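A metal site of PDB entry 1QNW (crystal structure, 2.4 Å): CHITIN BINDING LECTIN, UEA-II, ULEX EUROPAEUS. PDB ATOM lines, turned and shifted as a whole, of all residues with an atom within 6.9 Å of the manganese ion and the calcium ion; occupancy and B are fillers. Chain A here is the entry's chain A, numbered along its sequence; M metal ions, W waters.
The side-chain carboxylate (OD1) of Asp 139 sits close to the indole nitrogen (NE1) of Trp 138.
The side-chain hydroxyl of Ser 154 lies close to the side-chain carboxylate of Glu 126 (3.5 Å).
The backbone NH (N) of Glu 126 sits at hydrogen-bond distance from the backbone carbonyl oxygen (O) of Gly 146.
The side-chain carboxylate (OE1) of Glu 126 sits close to the side-chain carboxylate (OD2) of Asp 148.
A ring nitrogen (ND1) of His 144 lies within hydrogen-bond range of the backbone carbonyl oxygen (O) of Phe 142.
Of the 26 residues printed, 4 come within 4 Å of the manganese ion.
The nearest printed residue that does not touch the manganese ion is Ser 154 (4.4 Å).
Water W2 is bound to the manganese ion (2.0 Å).
The manganese ion is bound by OD2 of Asp 128.
A ring nitrogen (NE2) of His 144 binds the manganese ion (2.2 Å).
The side-chain carboxylate (OE2) of Glu 126 is bound to the manganese ion.
OD1 of Asp 139 binds the manganese ion, at 2.2 Å.
The manganese ion is bound by water W4, at 2.3 Å.
The calcium ion is bound by O of Tyr 130 (2.2 Å), OD1 of Asn 136 (2.3 Å), water W1 (2.4 Å), OD1 of Asp 128 (2.4 Å), water W3 (2.4 Å), OD2 of Asp 139 (2.4 Å) and OD2 of Asp 128 (2.6 Å).
The calcium ion has seven donor atoms within binding distance.
Water W4 lies within hydrogen-bond range of the side-chain carboxylate of Glu 126, the backbone carbonyl oxygen of Ile 152 and the indole nitrogen of Trp 138.
Water W3 bridges the backbone carbonyl oxygen of Gly 106 and the indole nitrogen of Trp 138.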
ATOM      1  N   ASP A  86     -10.687   4.079  -4.741  1.00  0.00           N
ATOM      2  CA  ASP A  86     -10.469   5.524  -4.779  1.00  0.00           C
ATOM      3  C   ASP A  86      -9.980   6.074  -3.441  1.00  0.00           C
ATOM      4  O   ASP A  86      -9.403   7.174  -3.375  1.00  0.00           O
ATOM      5  CB  ASP A  86     -11.777   6.232  -5.117  1.00  0.00           C
ATOM      6  CG  ASP A  86     -11.899   6.568  -6.579  1.00  0.00           C
ATOM      7  OD1 ASP A  86     -12.265   5.685  -7.378  1.00  0.00           O
ATOM      8  OD2 ASP A  86     -11.620   7.740  -6.923  1.00  0.00           O
ATOM      9  N   GLY A  87     -10.294   5.365  -2.366  1.00  0.00           N
ATOM     10  CA  GLY A  87      -9.876   5.842  -1.068  1.00  0.00           C
ATOM     11  C   GLY A  87     -10.880   5.560   0.035  1.00  0.00           C
ATOM     12  O   GLY A  87     -11.964   5.022  -0.208  1.00  0.00           O
ATOM     13  N   ALA A 105     -17.524   7.657  -6.449  1.00  0.00           N
ATOM     14  CA  ALA A 105     -16.474   7.039  -5.665  1.00  0.00           C
ATOM     15  C   ALA A 105     -15.394   8.053  -5.279  1.00  0.00           C
ATOM     16  O   ALA A 105     -14.849   7.996  -4.174  1.00  0.00           O
ATOM     17  CB  ALA A 105     -15.865   5.887  -6.423  1.00  0.00           C
ATOM     18  N   GLY A 106     -15.108   8.981  -6.200  1.00  0.00           N
ATOM     19  CA  GLY A 106     -14.107  10.009  -5.943  1.00  0.00           C
ATOM     20  C   GLY A 106     -14.510  11.027  -4.884  1.00  0.00           C
ATOM     21  O   GLY A 106     -13.699  11.845  -4.464  1.00  0.00           O
ATOM     22  N   MET A 107     -15.772  11.002  -4.493  1.00  0.00           N
ATOM     23  CA  MET A 107     -16.276  11.908  -3.484  1.00  0.00           C
ATOM     24  C   MET A 107     -16.643  11.129  -2.220  1.00  0.00           C
ATOM     25  O   MET A 107     -17.277  11.656  -1.303  1.00  0.00           O
ATOM     26  CB  MET A 107     -17.471  12.704  -4.018  1.00  0.00           C
ATOM     27  CG  MET A 107     -17.074  13.548  -5.214  1.00  0.00           C
ATOM     28  SD  MET A 107     -18.347  14.638  -5.799  1.00  0.00           S
ATOM     29  CE  MET A 107     -19.441  13.458  -6.605  1.00  0.00           C
ATOM     30  N   PHE A 108     -16.233   9.860  -2.196  1.00  0.00           N
ATOM     31  CA  PHE A 108     -16.431   8.948  -1.086  1.00  0.00           C
ATOM     32  C   PHE A 108     -17.866   8.842  -0.549  1.00  0.00           C
ATOM     33  O   PHE A 108     -18.080   8.543   0.628  1.00  0.00           O
ATOM     34  CB  PHE A 108     -15.454   9.278   0.046  1.00  0.00           C
ATOM     35  CG  PHE A 108     -14.044   9.499  -0.428  1.00  0.00           C
ATOM     36  CD1 PHE A 108     -13.310   8.453  -0.972  1.00  0.00           C
ATOM     37  CD2 PHE A 108     -13.473  10.770  -0.366  1.00  0.00           C
ATOM     38  CE1 PHE A 108     -12.021   8.663  -1.457  1.00  0.00           C
ATOM     39  CE2 PHE A 108     -12.186  10.990  -0.848  1.00  0.00           C
ATOM     40  CZ  PHE A 108     -11.462   9.941  -1.393  1.00  0.00           C
ATOM     41  N   GLU A 126      -9.781  12.290   4.762  1.00  0.00           N
ATOM     42  CA  GLU A 126      -9.664  11.340   3.665  1.00  0.00           C
ATOM     43  C   GLU A 126      -8.283  10.739   3.471  1.00  0.00           C
ATOM     44  O   GLU A 126      -7.267  11.373   3.722  1.00  0.00           O
ATOM     45  CB  GLU A 126     -10.104  12.002   2.363  1.00  0.00           C
ATOM     46  CG  GLU A 126      -9.317  13.251   2.041  1.00  0.00           C
ATOM     47  CD  GLU A 126      -9.521  13.721   0.629  1.00  0.00           C
ATOM     48  OE1 GLU A 126     -10.687  13.930   0.221  1.00  0.00           O
ATOM     49  OE2 GLU A 126      -8.521  13.863  -0.098  1.00  0.00           O
ATOM     50  N   PHE A 127      -8.279   9.494   3.032  1.00  0.00           N
ATOM     51  CA  PHE A 127      -7.055   8.769   2.734  1.00  0.00           C
ATOM     52  C   PHE A 127      -7.298   8.447   1.258  1.00  0.00           C
ATOM     53  O   PHE A 127      -7.868   7.422   0.901  1.00  0.00           O
ATOM     54  CB  PHE A 127      -6.951   7.522   3.620  1.00  0.00           C
ATOM     55  CG  PHE A 127      -6.968   7.845   5.091  1.00  0.00           C
ATOM     56  CD1 PHE A 127      -5.784   8.159   5.769  1.00  0.00           C
ATOM     57  CD2 PHE A 127      -8.172   7.922   5.790  1.00  0.00           C
ATOM     58  CE1 PHE A 127      -5.806   8.561   7.106  1.00  0.00           C
ATOM     59  CE2 PHE A 127      -8.205   8.328   7.139  1.00  0.00           C
ATOM     60  CZ  PHE A 127      -7.019   8.639   7.794  1.00  0.00           C
ATOM     61  N   ASP A 128      -6.965   9.446   0.439  1.00  0.00           N
ATOM     62  CA  ASP A 128      -7.145   9.461  -1.017  1.00  0.00           C
ATOM     63  C   ASP A 128      -6.056   8.771  -1.842  1.00  0.00           C
ATOM     64  O   ASP A 128      -4.940   9.268  -1.954  1.00  0.00           O
ATOM     65  CB  ASP A 128      -7.283  10.925  -1.448  1.00  0.00           C
ATOM     66  CG  ASP A 128      -8.038  11.103  -2.734  1.00  0.00           C
ATOM     67  OD1 ASP A 128      -8.146  10.154  -3.535  1.00  0.00           O
ATOM     68  OD2 ASP A 128      -8.510  12.228  -2.962  1.00  0.00           O
ATOM     69  N   THR A 129      -6.420   7.660  -2.487  1.00  0.00           N
ATOM     70  CA  THR A 129      -5.474   6.883  -3.302  1.00  0.00           C
ATOM     71  C   THR A 129      -5.450   7.257  -4.787  1.00  0.00           C
ATOM     72  O   THR A 129      -4.505   6.914  -5.502  1.00  0.00           O
ATOM     73  CB  THR A 129      -5.759   5.364  -3.190  1.00  0.00           C
ATOM     74  OG1 THR A 129      -7.119   5.098  -3.570  1.00  0.00           O
ATOM     75  CG2 THR A 129      -5.515   4.862  -1.777  1.00  0.00           C
ATOM     76  N   TYR A 130      -6.508   7.917  -5.268  1.00  0.00           N
ATOM     77  CA  TYR A 130      -6.588   8.313  -6.672  1.00  0.00           C
ATOM     78  C   TYR A 130      -6.580   9.824  -6.813  1.00  0.00           C
ATOM     79  O   TYR A 130      -7.436  10.521  -6.270  1.00  0.00           O
ATOM     80  CB  TYR A 130      -7.855   7.729  -7.319  1.00  0.00           C
ATOM     81  CG  TYR A 130      -8.063   8.181  -8.747  1.00  0.00           C
ATOM     82  CD1 TYR A 130      -7.314   7.638  -9.795  1.00  0.00           C
ATOM     83  CD2 TYR A 130      -8.996   9.183  -9.052  1.00  0.00           C
ATOM     84  CE1 TYR A 130      -7.494   8.076 -11.102  1.00  0.00           C
ATOM     85  CE2 TYR A 130      -9.177   9.623 -10.370  1.00  0.00           C
ATOM     86  CZ  TYR A 130      -8.427   9.070 -11.379  1.00  0.00           C
ATOM     87  OH  TYR A 130      -8.603   9.526 -12.671  1.00  0.00           O
ATOM     88  N   PHE A 131      -5.630  10.312  -7.598  1.00  0.00           N
ATOM     89  CA  PHE A 131      -5.482  11.747  -7.825  1.00  0.00           C
ATOM     90  C   PHE A 131      -5.417  12.123  -9.310  1.00  0.00           C
ATOM     91  O   PHE A 131      -4.938  13.214  -9.659  1.00  0.00           O
ATOM     92  CB  PHE A 131      -4.231  12.263  -7.103  1.00  0.00           C
ATOM     93  CG  PHE A 131      -2.976  11.513  -7.471  1.00  0.00           C
ATOM     94  CD1 PHE A 131      -2.636  10.329  -6.831  1.00  0.00           C
ATOM     95  CD2 PHE A 131      -2.138  11.998  -8.473  1.00  0.00           C
ATOM     96  CE1 PHE A 131      -1.479   9.632  -7.182  1.00  0.00           C
ATOM     97  CE2 PHE A 131      -0.984  11.313  -8.831  1.00  0.00           C
ATOM     98  CZ  PHE A 131      -0.653  10.124  -8.182  1.00  0.00           C
ATOM     99  N   GLY A 132      -5.890  11.229 -10.183  1.00  0.00           N
ATOM    100  CA  GLY A 132      -5.872  11.500 -11.613  1.00  0.00           C
ATOM    101  C   GLY A 132      -6.598  12.782 -11.969  1.00  0.00           C
ATOM    102  O   GLY A 132      -7.747  12.952 -11.578  1.00  0.00           O
ATOM    103  N   ASN A 136     -10.362  13.713 -10.933  1.00  0.00           N
ATOM    104  CA  ASN A 136     -10.176  14.436  -9.676  1.00  0.00           C
ATOM    105  C   ASN A 136      -9.247  15.630  -9.850  1.00  0.00           C
ATOM    106  O   ASN A 136      -8.160  15.673  -9.267  1.00  0.00           O
ATOM    107  CB  ASN A 136      -9.615  13.492  -8.590  1.00  0.00           C
ATOM    108  CG  ASN A 136     -10.630  12.439  -8.126  1.00  0.00           C
ATOM    109  OD1 ASN A 136     -10.303  11.570  -7.315  1.00  0.00           O
ATOM    110  ND2 ASN A 136     -11.836  12.515  -8.642  1.00  0.00           N
ATOM    111  N   TRP A 138      -9.325  18.471  -8.529  1.00  0.00           N
ATOM    112  CA  TRP A 138      -9.120  19.161  -7.251  1.00  0.00           C
ATOM    113  C   TRP A 138      -7.972  18.588  -6.414  1.00  0.00           C
ATOM    114  O   TRP A 138      -7.489  19.242  -5.484  1.00  0.00           O
ATOM    115  CB  TRP A 138     -10.411  19.111  -6.420  1.00  0.00           C
ATOM    116  CG  TRP A 138     -10.927  17.704  -6.251  1.00  0.00           C
ATOM    117  CD1 TRP A 138     -10.447  16.758  -5.392  1.00  0.00           C
ATOM    118  CD2 TRP A 138     -11.965  17.066  -7.011  1.00  0.00           C
ATOM    119  NE1 TRP A 138     -11.126  15.562  -5.566  1.00  0.00           N
ATOM    120  CE2 TRP A 138     -12.061  15.731  -6.550  1.00  0.00           C
ATOM    121  CE3 TRP A 138     -12.824  17.494  -8.028  1.00  0.00           C
ATOM    122  CZ2 TRP A 138     -12.984  14.814  -7.078  1.00  0.00           C
ATOM    123  CZ3 TRP A 138     -13.749  16.586  -8.553  1.00  0.00           C
ATOM    124  CH2 TRP A 138     -13.809  15.267  -8.078  1.00  0.00           C
ATOM    125  N   ASP A 139      -7.539  17.379  -6.728  1.00  0.00           N
ATOM    126  CA  ASP A 139      -6.478  16.689  -5.985  1.00  0.00           C
ATOM    127  C   ASP A 139      -5.050  17.080  -6.319  1.00  0.00           C
ATOM    128  O   ASP A 139      -4.766  17.561  -7.415  1.00  0.00           O
ATOM    129  CB  ASP A 139      -6.577  15.166  -6.199  1.00  0.00           C
ATOM    130  CG  ASP A 139      -7.635  14.528  -5.339  1.00  0.00           C
ATOM    131  OD1 ASP A 139      -8.009  15.106  -4.299  1.00  0.00           O
ATOM    132  OD2 ASP A 139      -8.101  13.429  -5.709  1.00  0.00           O
ATOM    133  N   PRO A 140      -4.131  16.897  -5.339  1.00  0.00           N
ATOM    134  CA  PRO A 140      -2.711  17.210  -5.517  1.00  0.00           C
ATOM    135  C   PRO A 140      -2.114  16.036  -6.322  1.00  0.00           C
ATOM    136  O   PRO A 140      -2.813  15.038  -6.566  1.00  0.00           O
ATOM    137  CB  PRO A 140      -2.184  17.261  -4.091  1.00  0.00           C
ATOM    138  CG  PRO A 140      -3.091  16.325  -3.358  1.00  0.00           C
ATOM    139  CD  PRO A 140      -4.435  16.686  -3.917  1.00  0.00           C
ATOM    140  N   PHE A 142      -0.291  13.377  -5.809  1.00  0.00           N
ATOM    141  CA  PHE A 142       0.188  12.232  -5.047  1.00  0.00           C
ATOM    142  C   PHE A 142      -0.915  11.706  -4.134  1.00  0.00           C
ATOM    143  O   PHE A 142      -1.919  12.368  -3.921  1.00  0.00           O
ATOM    144  CB  PHE A 142       1.414  12.620  -4.205  1.00  0.00           C
ATOM    145  CG  PHE A 142       1.280  13.938  -3.472  1.00  0.00           C
ATOM    146  CD1 PHE A 142       0.468  14.051  -2.346  1.00  0.00           C
ATOM    147  CD2 PHE A 142       1.963  15.062  -3.920  1.00  0.00           C
ATOM    148  CE1 PHE A 142       0.336  15.258  -1.675  1.00  0.00           C
ATOM    149  CE2 PHE A 142       1.838  16.284  -3.256  1.00  0.00           C
ATOM    150  CZ  PHE A 142       1.019  16.385  -2.132  1.00  0.00           C
ATOM    151  N   HIS A 144      -2.666  11.078  -0.829  1.00  0.00           N
ATOM    152  CA  HIS A 144      -2.609  11.995   0.297  1.00  0.00           C
ATOM    153  C   HIS A 144      -3.647  11.803   1.395  1.00  0.00           C
ATOM    154  O   HIS A 144      -4.608  11.055   1.257  1.00  0.00           O
ATOM    155  CB  HIS A 144      -2.791  13.414  -0.249  1.00  0.00           C
ATOM    156  CG  HIS A 144      -3.996  13.559  -1.120  1.00  0.00           C
ATOM    157  ND1 HIS A 144      -4.055  13.017  -2.391  1.00  0.00           N
ATOM    158  CD2 HIS A 144      -5.210  14.112  -0.891  1.00  0.00           C
ATOM    159  CE1 HIS A 144      -5.252  13.247  -2.907  1.00  0.00           C
ATOM    160  NE2 HIS A 144      -5.970  13.897  -2.016  1.00  0.00           N
ATOM    161  N   ILE A 145      -3.422  12.530   2.486  1.00  0.00           N
ATOM    162  CA  ILE A 145      -4.329  12.569   3.625  1.00  0.00           C
ATOM    163  C   ILE A 145      -4.861  13.995   3.533  1.00  0.00           C
ATOM    164  O   ILE A 145      -4.084  14.940   3.397  1.00  0.00           O
ATOM    165  CB  ILE A 145      -3.608  12.383   4.982  1.00  0.00           C
ATOM    166  CG1 ILE A 145      -2.964  11.007   5.054  1.00  0.00           C
ATOM    167  CG2 ILE A 145      -4.608  12.532   6.132  1.00  0.00           C
ATOM    168  CD1 ILE A 145      -2.136  10.800   6.288  1.00  0.00           C
ATOM    169  N   GLY A 146      -6.181  14.149   3.539  1.00  0.00           N
ATOM    170  CA  GLY A 146      -6.729  15.484   3.443  1.00  0.00           C
ATOM    171  C   GLY A 146      -7.791  15.765   4.486  1.00  0.00           C
ATOM    172  O   GLY A 146      -8.448  14.843   4.969  1.00  0.00           O
ATOM    173  N   ASP A 148     -11.136  17.579   4.857  1.00  0.00           N
ATOM    174  CA  ASP A 148     -12.214  18.122   4.043  1.00  0.00           C
ATOM    175  C   ASP A 148     -13.248  18.832   4.893  1.00  0.00           C
ATOM    176  O   ASP A 148     -13.744  18.283   5.861  1.00  0.00           O
ATOM    177  CB  ASP A 148     -12.893  17.010   3.269  1.00  0.00           C
ATOM    178  CG  ASP A 148     -11.952  16.271   2.350  1.00  0.00           C
ATOM    179  OD1 ASP A 148     -10.808  16.725   2.153  1.00  0.00           O
ATOM    180  OD2 ASP A 148     -12.363  15.241   1.791  1.00  0.00           O
ATOM    181  N   ILE A 152     -14.928  18.388  -1.354  1.00  0.00           N
ATOM    182  CA  ILE A 152     -14.025  17.288  -1.688  1.00  0.00           C
ATOM    183  C   ILE A 152     -12.625  17.841  -1.934  1.00  0.00           C
ATOM    184  O   ILE A 152     -11.634  17.111  -1.959  1.00  0.00           O
ATOM    185  CB  ILE A 152     -14.536  16.498  -2.926  1.00  0.00           C
ATOM    186  CG1 ILE A 152     -13.753  15.192  -3.075  1.00  0.00           C
ATOM    187  CG2 ILE A 152     -14.418  17.351  -4.175  1.00  0.00           C
ATOM    188  CD1 ILE A 152     -13.867  14.261  -1.889  1.00  0.00           C
ATOM    189  N   LYS A 153     -12.541  19.163  -2.129  1.00  0.00           N
ATOM    190  CA  LYS A 153     -11.284  19.849  -2.346  1.00  0.00           C
ATOM    191  C   LYS A 153     -10.772  20.229  -0.953  1.00  0.00           C
ATOM    192  O   LYS A 153     -11.222  21.214  -0.359  1.00  0.00           O
ATOM    193  CB  LYS A 153     -11.515  21.096  -3.210  1.00  0.00           C
ATOM    194  CG  LYS A 153     -10.273  21.928  -3.500  1.00  0.00           C
ATOM    195  CD  LYS A 153     -10.611  23.120  -4.397  1.00  0.00           C
ATOM    196  CE  LYS A 153      -9.469  24.119  -4.463  1.00  0.00           C
ATOM    197  NZ  LYS A 153      -8.215  23.469  -4.917  1.00  0.00           N
ATOM    198  N   SER A 154      -9.879  19.396  -0.412  1.00  0.00           N
ATOM    199  CA  SER A 154      -9.293  19.556   0.919  1.00  0.00           C
ATOM    200  C   SER A 154      -8.744  20.934   1.229  1.00  0.00           C
ATOM    201  O   SER A 154      -8.073  21.541   0.389  1.00  0.00           O
ATOM    202  CB  SER A 154      -8.173  18.542   1.114  1.00  0.00           C
ATOM    203  OG  SER A 154      -8.584  17.241   0.749  1.00  0.00           O
ATOM    204  N   THR A 157      -3.755  19.237   2.780  1.00  0.00           N
ATOM    205  CA  THR A 157      -3.350  17.860   2.493  1.00  0.00           C
ATOM    206  C   THR A 157      -1.891  17.654   2.854  1.00  0.00           C
ATOM    207  O   THR A 157      -1.159  18.605   3.105  1.00  0.00           O
ATOM    208  CB  THR A 157      -3.516  17.490   1.002  1.00  0.00           C
ATOM    209  OG1 THR A 157      -2.635  18.302   0.225  1.00  0.00           O
ATOM    210  CG2 THR A 157      -4.938  17.664   0.527  1.00  0.00           C
HETATM  211 MN    MN M   1      -8.120  14.142  -2.271  1.00  0.00          MN
HETATM  212 CA    CA M   2      -9.248  11.345  -5.249  1.00  0.00          CA
HETATM  213  O   HOH W   1     -10.179   9.197  -4.988  1.00  0.00           O
HETATM  214  O   HOH W   2      -7.885  16.004  -1.705  1.00  0.00           O
HETATM  215  O   HOH W   3     -11.128  12.624  -4.494  1.00  0.00           O
HETATM  216  O   HOH W   4     -10.375  14.602  -2.474  1.00  0.00           O
